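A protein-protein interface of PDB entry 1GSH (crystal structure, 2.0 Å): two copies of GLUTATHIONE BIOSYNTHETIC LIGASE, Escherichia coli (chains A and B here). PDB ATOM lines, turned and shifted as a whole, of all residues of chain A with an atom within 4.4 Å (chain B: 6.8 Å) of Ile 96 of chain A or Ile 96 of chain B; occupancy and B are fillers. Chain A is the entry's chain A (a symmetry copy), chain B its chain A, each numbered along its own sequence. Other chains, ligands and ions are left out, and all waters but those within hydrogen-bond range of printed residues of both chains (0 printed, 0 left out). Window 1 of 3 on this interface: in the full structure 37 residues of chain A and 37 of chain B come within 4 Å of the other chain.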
ATOM      1  N   PHE A  91      18.993  -9.860 -20.274  1.00  0.00           N
ATOM      2  CA  PHE A  91      18.671  -8.460 -20.194  1.00  0.00           C
ATOM      3  C   PHE A  91      17.528  -8.427 -19.171  1.00  0.00           C
ATOM      4  O   PHE A  91      16.374  -8.761 -19.454  1.00  0.00           O
ATOM      5  CB  PHE A  91      18.200  -7.954 -21.542  1.00  0.00           C
ATOM      6  CG  PHE A  91      18.000  -6.451 -21.514  1.00  0.00           C
ATOM      7  CD1 PHE A  91      19.103  -5.618 -21.285  1.00  0.00           C
ATOM      8  CD2 PHE A  91      16.724  -5.919 -21.729  1.00  0.00           C
ATOM      9  CE1 PHE A  91      18.932  -4.234 -21.250  1.00  0.00           C
ATOM     10  CE2 PHE A  91      16.569  -4.532 -21.694  1.00  0.00           C
ATOM     11  CZ  PHE A  91      17.668  -3.688 -21.457  1.00  0.00           C
ATOM     12  N   ASP A  92      17.886  -8.071 -17.948  1.00  0.00           N
ATOM     13  CA  ASP A  92      16.942  -8.055 -16.863  1.00  0.00           C
ATOM     14  C   ASP A  92      16.947  -6.672 -16.244  1.00  0.00           C
ATOM     15  O   ASP A  92      17.650  -5.779 -16.742  1.00  0.00           O
ATOM     16  CB  ASP A  92      17.354  -9.169 -15.863  1.00  0.00           C
ATOM     17  CG  ASP A  92      18.729  -9.073 -15.163  1.00  0.00           C
ATOM     18  OD1 ASP A  92      19.477  -8.122 -15.363  1.00  0.00           O
ATOM     19  OD2 ASP A  92      19.068  -9.960 -14.385  1.00  0.00           O
ATOM     20  N   THR A  93      16.213  -6.465 -15.145  1.00  0.00           N
ATOM     21  CA  THR A  93      16.158  -5.145 -14.526  1.00  0.00           C
ATOM     22  C   THR A  93      17.488  -4.728 -13.914  1.00  0.00           C
ATOM     23  O   THR A  93      17.776  -3.538 -13.967  1.00  0.00           O
ATOM     24  CB  THR A  93      15.037  -5.062 -13.426  1.00  0.00           C
ATOM     25  OG1 THR A  93      15.064  -6.233 -12.603  1.00  0.00           O
ATOM     26  CG2 THR A  93      13.679  -4.880 -14.095  1.00  0.00           C
ATOM     27  N   GLU A  94      18.325  -5.655 -13.409  1.00  0.00           N
ATOM     28  CA  GLU A  94      19.658  -5.330 -12.901  1.00  0.00           C
ATOM     29  C   GLU A  94      20.546  -4.790 -14.011  1.00  0.00           C
ATOM     30  O   GLU A  94      21.286  -3.822 -13.812  1.00  0.00           O
ATOM     31  CB  GLU A  94      20.341  -6.551 -12.315  1.00  0.00           C
ATOM     32  CG  GLU A  94      19.716  -7.108 -11.045  1.00  0.00           C
ATOM     33  CD  GLU A  94      19.638  -6.079  -9.906  1.00  0.00           C
ATOM     34  OE1 GLU A  94      20.656  -5.542  -9.461  1.00  0.00           O
ATOM     35  OE2 GLU A  94      18.534  -5.801  -9.462  1.00  0.00           O
ATOM     36  N   PHE A  95      20.439  -5.381 -15.209  1.00  0.00           N
ATOM     37  CA  PHE A  95      21.186  -4.933 -16.358  1.00  0.00           C
ATOM     38  C   PHE A  95      20.712  -3.514 -16.625  1.00  0.00           C
ATOM     39  O   PHE A  95      21.538  -2.621 -16.760  1.00  0.00           O
ATOM     40  CB  PHE A  95      20.874  -5.831 -17.542  1.00  0.00           C
ATOM     41  CG  PHE A  95      21.901  -5.680 -18.649  1.00  0.00           C
ATOM     42  CD1 PHE A  95      21.966  -4.510 -19.404  1.00  0.00           C
ATOM     43  CD2 PHE A  95      22.818  -6.701 -18.849  1.00  0.00           C
ATOM     44  CE1 PHE A  95      22.964  -4.346 -20.354  1.00  0.00           C
ATOM     45  CE2 PHE A  95      23.813  -6.526 -19.805  1.00  0.00           C
ATOM     46  CZ  PHE A  95      23.885  -5.354 -20.546  1.00  0.00           C
ATOM     47  N   ILE A  96      19.390  -3.280 -16.668  1.00  0.00           N
ATOM     48  CA  ILE A  96      18.857  -1.929 -16.855  1.00  0.00           C
ATOM     49  C   ILE A  96      19.301  -0.930 -15.789  1.00  0.00           C
ATOM     50  O   ILE A  96      19.598   0.221 -16.131  1.00  0.00           O
ATOM     51  CB  ILE A  96      17.312  -2.022 -16.918  1.00  0.00           C
ATOM     52  CG1 ILE A  96      17.018  -2.623 -18.267  1.00  0.00           C
ATOM     53  CG2 ILE A  96      16.598  -0.688 -16.747  1.00  0.00           C
ATOM     54  CD1 ILE A  96      15.789  -3.496 -18.233  1.00  0.00           C
ATOM     55  N   TYR A  97      19.385  -1.307 -14.512  1.00  0.00           N
ATOM     56  CA  TYR A  97      19.890  -0.384 -13.485  1.00  0.00           C
ATOM     57  C   TYR A  97      21.368  -0.037 -13.681  1.00  0.00           C
ATOM     58  O   TYR A  97      21.719   1.142 -13.553  1.00  0.00           O
ATOM     59  CB  TYR A  97      19.719  -0.975 -12.074  1.00  0.00           C
ATOM     60  CG  TYR A  97      18.262  -1.268 -11.718  1.00  0.00           C
ATOM     61  CD1 TYR A  97      17.236  -0.404 -12.125  1.00  0.00           C
ATOM     62  CD2 TYR A  97      17.943  -2.424 -10.984  1.00  0.00           C
ATOM     63  CE1 TYR A  97      15.916  -0.696 -11.803  1.00  0.00           C
ATOM     64  CE2 TYR A  97      16.622  -2.712 -10.673  1.00  0.00           C
ATOM     65  CZ  TYR A  97      15.618  -1.846 -11.081  1.00  0.00           C
ATOM     66  OH  TYR A  97      14.295  -2.120 -10.783  1.00  0.00           O
ATOM     67  N   ALA A  98      22.231  -1.007 -14.070  1.00  0.00           N
ATOM     68  CA  ALA A  98      23.653  -0.759 -14.314  1.00  0.00           C
ATOM     69  C   ALA A  98      23.870   0.220 -15.448  1.00  0.00           C
ATOM     70  O   ALA A  98      24.819   0.996 -15.493  1.00  0.00           O
ATOM     71  CB  ALA A  98      24.363  -2.036 -14.677  1.00  0.00           C
ATOM     72  N   THR A  99      22.959   0.163 -16.405  1.00  0.00           N
ATOM     73  CA  THR A  99      22.894   1.078 -17.523  1.00  0.00           C
ATOM     74  C   THR A  99      22.760   2.536 -17.053  1.00  0.00           C
ATOM     75  O   THR A  99      23.377   3.442 -17.619  1.00  0.00           O
ATOM     76  CB  THR A  99      21.716   0.471 -18.281  1.00  0.00           C
ATOM     77  OG1 THR A  99      22.261  -0.287 -19.359  1.00  0.00           O
ATOM     78  CG2 THR A  99      20.720   1.459 -18.663  1.00  0.00           C
ATOM     79  N   TYR A 100      21.990   2.822 -15.984  1.00  0.00           N
ATOM     80  CA  TYR A 100      21.818   4.195 -15.497  1.00  0.00           C
ATOM     81  C   TYR A 100      23.071   4.661 -14.787  1.00  0.00           C
ATOM     82  O   TYR A 100      23.400   5.846 -14.804  1.00  0.00           O
ATOM     83  CB  TYR A 100      20.663   4.304 -14.508  1.00  0.00           C
ATOM     84  CG  TYR A 100      19.294   3.852 -15.036  1.00  0.00           C
ATOM     85  CD1 TYR A 100      18.772   4.318 -16.247  1.00  0.00           C
ATOM     86  CD2 TYR A 100      18.536   2.983 -14.261  1.00  0.00           C
ATOM     87  CE1 TYR A 100      17.489   3.929 -16.652  1.00  0.00           C
ATOM     88  CE2 TYR A 100      17.261   2.598 -14.661  1.00  0.00           C
ATOM     89  CZ  TYR A 100      16.738   3.073 -15.858  1.00  0.00           C
ATOM     90  OH  TYR A 100      15.433   2.732 -16.206  1.00  0.00           O
ATOM     91  N   MET B  40      -2.493  -5.295 -20.758  1.00  0.00           N
ATOM     92  CA  MET B  40      -1.192  -5.648 -21.313  1.00  0.00           C
ATOM     93  C   MET B  40      -1.250  -6.787 -22.313  1.00  0.00           C
ATOM     94  O   MET B  40      -0.629  -6.762 -23.375  1.00  0.00           O
ATOM     95  CB  MET B  40      -0.226  -6.078 -20.208  1.00  0.00           C
ATOM     96  CG  MET B  40       0.163  -5.021 -19.219  1.00  0.00           C
ATOM     97  SD  MET B  40       1.357  -3.883 -19.934  1.00  0.00           S
ATOM     98  CE  MET B  40       2.756  -4.924 -19.616  1.00  0.00           C
ATOM     99  N   PHE B  91       8.008  -2.024 -12.329  1.00  0.00           N
ATOM    100  CA  PHE B  91       8.699  -1.741 -13.559  1.00  0.00           C
ATOM    101  C   PHE B  91       9.577  -2.984 -13.755  1.00  0.00           C
ATOM    102  O   PHE B  91      10.615  -3.171 -13.116  1.00  0.00           O
ATOM    103  CB  PHE B  91       9.554  -0.500 -13.403  1.00  0.00           C
ATOM    104  CG  PHE B  91      10.172  -0.100 -14.729  1.00  0.00           C
ATOM    105  CD1 PHE B  91       9.336   0.280 -15.786  1.00  0.00           C
ATOM    106  CD2 PHE B  91      11.564  -0.106 -14.873  1.00  0.00           C
ATOM    107  CE1 PHE B  91       9.891   0.644 -17.014  1.00  0.00           C
ATOM    108  CE2 PHE B  91      12.104   0.262 -16.106  1.00  0.00           C
ATOM    109  CZ  PHE B  91      11.274   0.639 -17.176  1.00  0.00           C
ATOM    110  N   ASP B  92       9.103  -3.869 -14.618  1.00  0.00           N
ATOM    111  CA  ASP B  92       9.776  -5.115 -14.862  1.00  0.00           C
ATOM    112  C   ASP B  92      10.050  -5.228 -16.349  1.00  0.00           C
ATOM    113  O   ASP B  92       9.749  -4.289 -17.101  1.00  0.00           O
ATOM    114  CB  ASP B  92       8.869  -6.255 -14.324  1.00  0.00           C
ATOM    115  CG  ASP B  92       7.471  -6.456 -14.953  1.00  0.00           C
ATOM    116  OD1 ASP B  92       7.086  -5.754 -15.882  1.00  0.00           O
ATOM    117  OD2 ASP B  92       6.742  -7.345 -14.519  1.00  0.00           O
ATOM    118  N   THR B  93      10.579  -6.365 -16.812  1.00  0.00           N
ATOM    119  CA  THR B  93      10.892  -6.515 -18.230  1.00  0.00           C
ATOM    120  C   THR B  93       9.646  -6.548 -19.104  1.00  0.00           C
ATOM    121  O   THR B  93       9.732  -6.035 -20.213  1.00  0.00           O
ATOM    122  CB  THR B  93      11.748  -7.806 -18.505  1.00  0.00           C
ATOM    123  OG1 THR B  93      11.219  -8.916 -17.772  1.00  0.00           O
ATOM    124  CG2 THR B  93      13.204  -7.539 -18.143  1.00  0.00           C
ATOM    125  N   GLU B  94       8.494  -7.058 -18.629  1.00  0.00           N
ATOM    126  CA  GLU B  94       7.239  -7.025 -19.381  1.00  0.00           C
ATOM    127  C   GLU B  94       6.785  -5.593 -19.617  1.00  0.00           C
ATOM    128  O   GLU B  94       6.333  -5.247 -20.712  1.00  0.00           O
ATOM    129  CB  GLU B  94       6.130  -7.747 -18.640  1.00  0.00           C
ATOM    130  CG  GLU B  94       6.302  -9.251 -18.503  1.00  0.00           C
ATOM    131  CD  GLU B  94       6.447  -9.971 -19.854  1.00  0.00           C
ATOM    132  OE1 GLU B  94       5.561  -9.905 -20.711  1.00  0.00           O
ATOM    133  OE2 GLU B  94       7.473 -10.603 -20.056  1.00  0.00           O
ATOM    134  N   PHE B  95       6.950  -4.734 -18.602  1.00  0.00           N
ATOM    135  CA  PHE B  95       6.609  -3.337 -18.712  1.00  0.00           C
ATOM    136  C   PHE B  95       7.517  -2.779 -19.795  1.00  0.00           C
ATOM    137  O   PHE B  95       7.028  -2.131 -20.712  1.00  0.00           O
ATOM    138  CB  PHE B  95       6.873  -2.649 -17.385  1.00  0.00           C
ATOM    139  CG  PHE B  95       6.176  -1.305 -17.299  1.00  0.00           C
ATOM    140  CD1 PHE B  95       6.604  -0.229 -18.076  1.00  0.00           C
ATOM    141  CD2 PHE B  95       5.061  -1.185 -16.483  1.00  0.00           C
ATOM    142  CE1 PHE B  95       5.906   0.970 -18.056  1.00  0.00           C
ATOM    143  CE2 PHE B  95       4.370   0.021 -16.470  1.00  0.00           C
ATOM    144  CZ  PHE B  95       4.788   1.086 -17.256  1.00  0.00           C
ATOM    145  N   ILE B  96       8.831  -3.049 -19.727  1.00  0.00           N
ATOM    146  CA  ILE B  96       9.758  -2.601 -20.768  1.00  0.00           C
ATOM    147  C   ILE B  96       9.423  -3.113 -22.166  1.00  0.00           C
ATOM    148  O   ILE B  96       9.546  -2.349 -23.132  1.00  0.00           O
ATOM    149  CB  ILE B  96      11.191  -3.022 -20.353  1.00  0.00           C
ATOM    150  CG1 ILE B  96      11.560  -2.084 -19.235  1.00  0.00           C
ATOM    151  CG2 ILE B  96      12.212  -2.956 -21.481  1.00  0.00           C
ATOM    152  CD1 ILE B  96      12.449  -2.752 -18.217  1.00  0.00           C
ATOM    153  N   TYR B  97       8.981  -4.361 -22.335  1.00  0.00           N
ATOM    154  CA  TYR B  97       8.573  -4.844 -23.661  1.00  0.00           C
ATOM    155  C   TYR B  97       7.328  -4.127 -24.191  1.00  0.00           C
ATOM    156  O   TYR B  97       7.317  -3.762 -25.373  1.00  0.00           O
ATOM    157  CB  TYR B  97       8.282  -6.356 -23.638  1.00  0.00           C
ATOM    158  CG  TYR B  97       9.490  -7.193 -23.222  1.00  0.00           C
ATOM    159  CD1 TYR B  97      10.783  -6.847 -23.641  1.00  0.00           C
ATOM    160  CD2 TYR B  97       9.308  -8.318 -22.399  1.00  0.00           C
ATOM    161  CE1 TYR B  97      11.870  -7.613 -23.240  1.00  0.00           C
ATOM    162  CE2 TYR B  97      10.399  -9.075 -21.997  1.00  0.00           C
ATOM    163  CZ  TYR B  97      11.672  -8.720 -22.422  1.00  0.00           C
ATOM    164  OH  TYR B  97      12.772  -9.461 -22.028  1.00  0.00           O
ATOM    165  N   ALA B  98       6.316  -3.838 -23.338  1.00  0.00           N
ATOM    166  CA  ALA B  98       5.105  -3.125 -23.749  1.00  0.00           C
ATOM    167  C   ALA B  98       5.410  -1.725 -24.239  1.00  0.00           C
ATOM    168  O   ALA B  98       4.756  -1.160 -25.110  1.00  0.00           O
ATOM    169  CB  ALA B  98       4.141  -3.001 -22.600  1.00  0.00           C
ATOM    170  N   THR B  99       6.436  -1.145 -23.639  1.00  0.00           N
ATOM    171  CA  THR B  99       6.985   0.137 -24.022  1.00  0.00           C
ATOM    172  C   THR B  99       7.440   0.143 -25.490  1.00  0.00           C
ATOM    173  O   THR B  99       7.237   1.124 -26.212  1.00  0.00           O
ATOM    174  CB  THR B  99       8.061   0.284 -22.949  1.00  0.00           C
ATOM    175  OG1 THR B  99       7.545   1.171 -21.959  1.00  0.00           O
ATOM    176  CG2 THR B  99       9.356   0.658 -23.496  1.00  0.00           C
ATOM    177  N   TYR B 100       8.032  -0.952 -26.007  1.00  0.00           N
ATOM    178  CA  TYR B 100       8.495  -1.001 -27.397  1.00  0.00           C
ATOM    179  C   TYR B 100       7.317  -1.128 -28.340  1.00  0.00           C
ATOM    180  O   TYR B 100       7.355  -0.636 -29.466  1.00  0.00           O
ATOM    181  CB  TYR B 100       9.412  -2.193 -27.647  1.00  0.00           C
ATOM    182  CG  TYR B 100      10.666  -2.258 -26.766  1.00  0.00           C
ATOM    183  CD1 TYR B 100      11.530  -1.169 -26.617  1.00  0.00           C
ATOM    184  CD2 TYR B 100      10.971  -3.457 -26.131  1.00  0.00           C
ATOM    185  CE1 TYR B 100      12.699  -1.302 -25.856  1.00  0.00           C
ATOM    186  CE2 TYR B 100      12.132  -3.590 -25.377  1.00  0.00           C
ATOM    187  CZ  TYR B 100      12.997  -2.509 -25.241  1.00  0.00           C
ATOM    188  OH  TYR B 100      14.189  -2.684 -24.542  1.00  0.00           O
ATOM    189  N   ILE B 101       6.254  -1.782 -27.856  1.00  0.00           N
ATOM    190  CA  ILE B 101       5.025  -1.924 -28.627  1.00  0.00           C
ATOM    191  C   ILE B 101       4.358  -0.555 -28.739  1.00  0.00           C
ATOM    192  O   ILE B 101       4.009  -0.104 -29.833  1.00  0.00           O
ATOM    193  CB  ILE B 101       4.125  -2.970 -27.914  1.00  0.00           C
ATOM    194  CG1 ILE B 101       4.770  -4.351 -27.983  1.00  0.00           C
ATOM    195  CG2 ILE B 101       2.754  -2.991 -28.558  1.00  0.00           C
ATOM    196  CD1 ILE B 101       4.001  -5.427 -27.192  1.00  0.00           C
ATOM    197  N   LEU B 119       9.880   6.475 -20.250  1.00  0.00           N
ATOM    198  CA  LEU B 119       9.548   5.486 -19.231  1.00  0.00           C
ATOM    199  C   LEU B 119      10.710   4.520 -18.955  1.00  0.00           C
ATOM    200  O   LEU B 119      10.865   4.013 -17.829  1.00  0.00           O
ATOM    201  CB  LEU B 119       8.310   4.692 -19.685  1.00  0.00           C
ATOM    202  CG  LEU B 119       6.976   5.435 -19.726  1.00  0.00           C
ATOM    203  CD1 LEU B 119       5.847   4.510 -20.212  1.00  0.00           C
ATOM    204  CD2 LEU B 119       6.681   5.954 -18.329  1.00  0.00           C
ATOM    205  N   ARG B 120      11.524   4.245 -19.990  1.00  0.00           N
ATOM    206  CA  ARG B 120      12.690   3.389 -19.858  1.00  0.00           C
ATOM    207  C   ARG B 120      13.878   4.150 -19.284  1.00  0.00           C
ATOM    208  O   ARG B 120      14.670   3.589 -18.544  1.00  0.00           O
ATOM    209  CB  ARG B 120      13.113   2.817 -21.216  1.00  0.00           C
ATOM    210  CG  ARG B 120      12.160   1.794 -21.797  1.00  0.00           C
ATOM    211  CD  ARG B 120      12.733   1.158 -23.072  1.00  0.00           C
ATOM    212  NE  ARG B 120      13.110   2.130 -24.088  1.00  0.00           N
ATOM    213  CZ  ARG B 120      12.344   2.465 -25.147  1.00  0.00           C
ATOM    214  NH1 ARG B 120      11.166   1.941 -25.420  1.00  0.00           N
ATOM    215  NH2 ARG B 120      12.827   3.274 -26.074  1.00  0.00           N
ATOM    216  N   ASN B 123      13.743   5.967 -14.394  1.00  0.00           N
ATOM    217  CA  ASN B 123      13.313   5.074 -13.337  1.00  0.00           C
ATOM    218  C   ASN B 123      12.790   5.937 -12.184  1.00  0.00           C
ATOM    219  O   ASN B 123      13.351   6.989 -11.859  1.00  0.00           O
ATOM    220  CB  ASN B 123      14.478   4.221 -12.837  1.00  0.00           C
ATOM    221  CG  ASN B 123      14.058   3.233 -11.774  1.00  0.00           C
ATOM    222  OD1 ASN B 123      14.407   3.329 -10.605  1.00  0.00           O
ATOM    223  ND2 ASN B 123      13.280   2.231 -12.146  1.00  0.00           N
ATOM    224  N   LEU B 126      15.645   5.790  -9.451  1.00  0.00           N
ATOM    225  CA  LEU B 126      16.959   6.201  -9.900  1.00  0.00           C
ATOM    226  C   LEU B 126      17.027   7.490 -10.680  1.00  0.00           C
ATOM    227  O   LEU B 126      18.115   8.063 -10.776  1.00  0.00           O
ATOM    228  CB  LEU B 126      17.556   5.087 -10.725  1.00  0.00           C
ATOM    229  CG  LEU B 126      18.555   4.200 -10.014  1.00  0.00           C
ATOM    230  CD1 LEU B 126      18.057   3.779  -8.663  1.00  0.00           C
ATOM    231  CD2 LEU B 126      18.737   2.957 -10.813  1.00  0.00           C
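OH of Tyr 100 of chain A sits at hydrogen-bond distance from O of Arg 120 of chain B (2.6 Å).
The side-chain carboxylate of Asp 92 of chain B lies close to the backbone NH of Glu 94 of chain B, at 3.4 Å. The side-chain carboxylate (OD1) of Asp 92 of chain B is in hydrogen-bond range of the backbone NH (N) of Phe 95 of chain B (2.9 Å). The backbone NH (N) of Leu 126 of chain B is in hydrogen-bond range of the side-chain amide oxygen (OD1) of Asn 123 of chain B, at 3.0 Å. The backbone NH of Glu 94 of chain A sits close to the side-chain carboxylate of Asp 92 of chain A, 3.4 Å away. N of Phe 95 of chain A lies within hydrogen-bond range of OD1 of Asp 92 of chain A (2.9 Å).
O of Phe 91 of chain A touches CG2 of Thr 93 of chain B, at 3.6 Å. Asp 92 of chain A touches Thr 93 of chain B. Thr 93 of chain A touches Phe 91 of chain B (CG2 to O, 3.6 Å). Thr 93 of chain A touches Asp 92 of chain B (CG2 to CA, 3.98 Å). Ile 96 of chain A touches Ile 96 of chain B. Asn 123 of chain B touches Tyr 97 of chain A (ND2 to CE1, 3.95 Å). Leu 126 of chain B touches Tyr 97 of chain A. Tyr 100 of chain A touches Asn 123 of chain B. CD2 of Tyr 100 of chain A touches CD2 of Leu 126 of chain B, at 3.5 Å.
Of the printed residues of chain B, Asp 92 of chain A touches Thr 93. Of the printed residues of chain B, Thr 93 of chain A touches Phe 91 and Asp 92. Glu 94 of chain A touches none of the printed residues of chain B. Ile 96 of chain A touches one residue of chain B. Printed residues of chain B within 4 Å of Tyr 100 of chain A: Arg 120, Asn 123 and Leu 126. Printed residues of chain A within 4 Å of Phe 91 of chain B: Thr 93. Phe 95 of chain B touches none of the printed residues of chain A. Printed residues of chain A within 4 Å of Asn 123 of chain B: Tyr 97 and Tyr 100. The nearest residue of chain B that does not touch Ile 96 of chain A is Phe 91 of chain B (4.6 Å).
Printed residues of chain A that touch a printed residue of chain B: Phe 91, Asp 92, Thr 93, Ile 96, Tyr 97 and Tyr 100. Hydrophobic or aromatic side chains of chain B within 4 Å of the printed part of chain A: Ile 96 and Leu 126.
Phe 91 of chain A touches Thr 93 of chain B, and with the chains exchanged Thr 93 of chain A touches Phe 91 of chain B. Asp 92 of chain A touches Thr 93 of chain B, and with the chains exchanged Thr 93 of chain A touches Asp 92 of chain B. Ile 96 of chain B touches its own counterpart, Ile 96 of chain A. Positions printed for both chains: 91, 92, 93, 94, 95, 96, 97, 98, 99 and 100.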
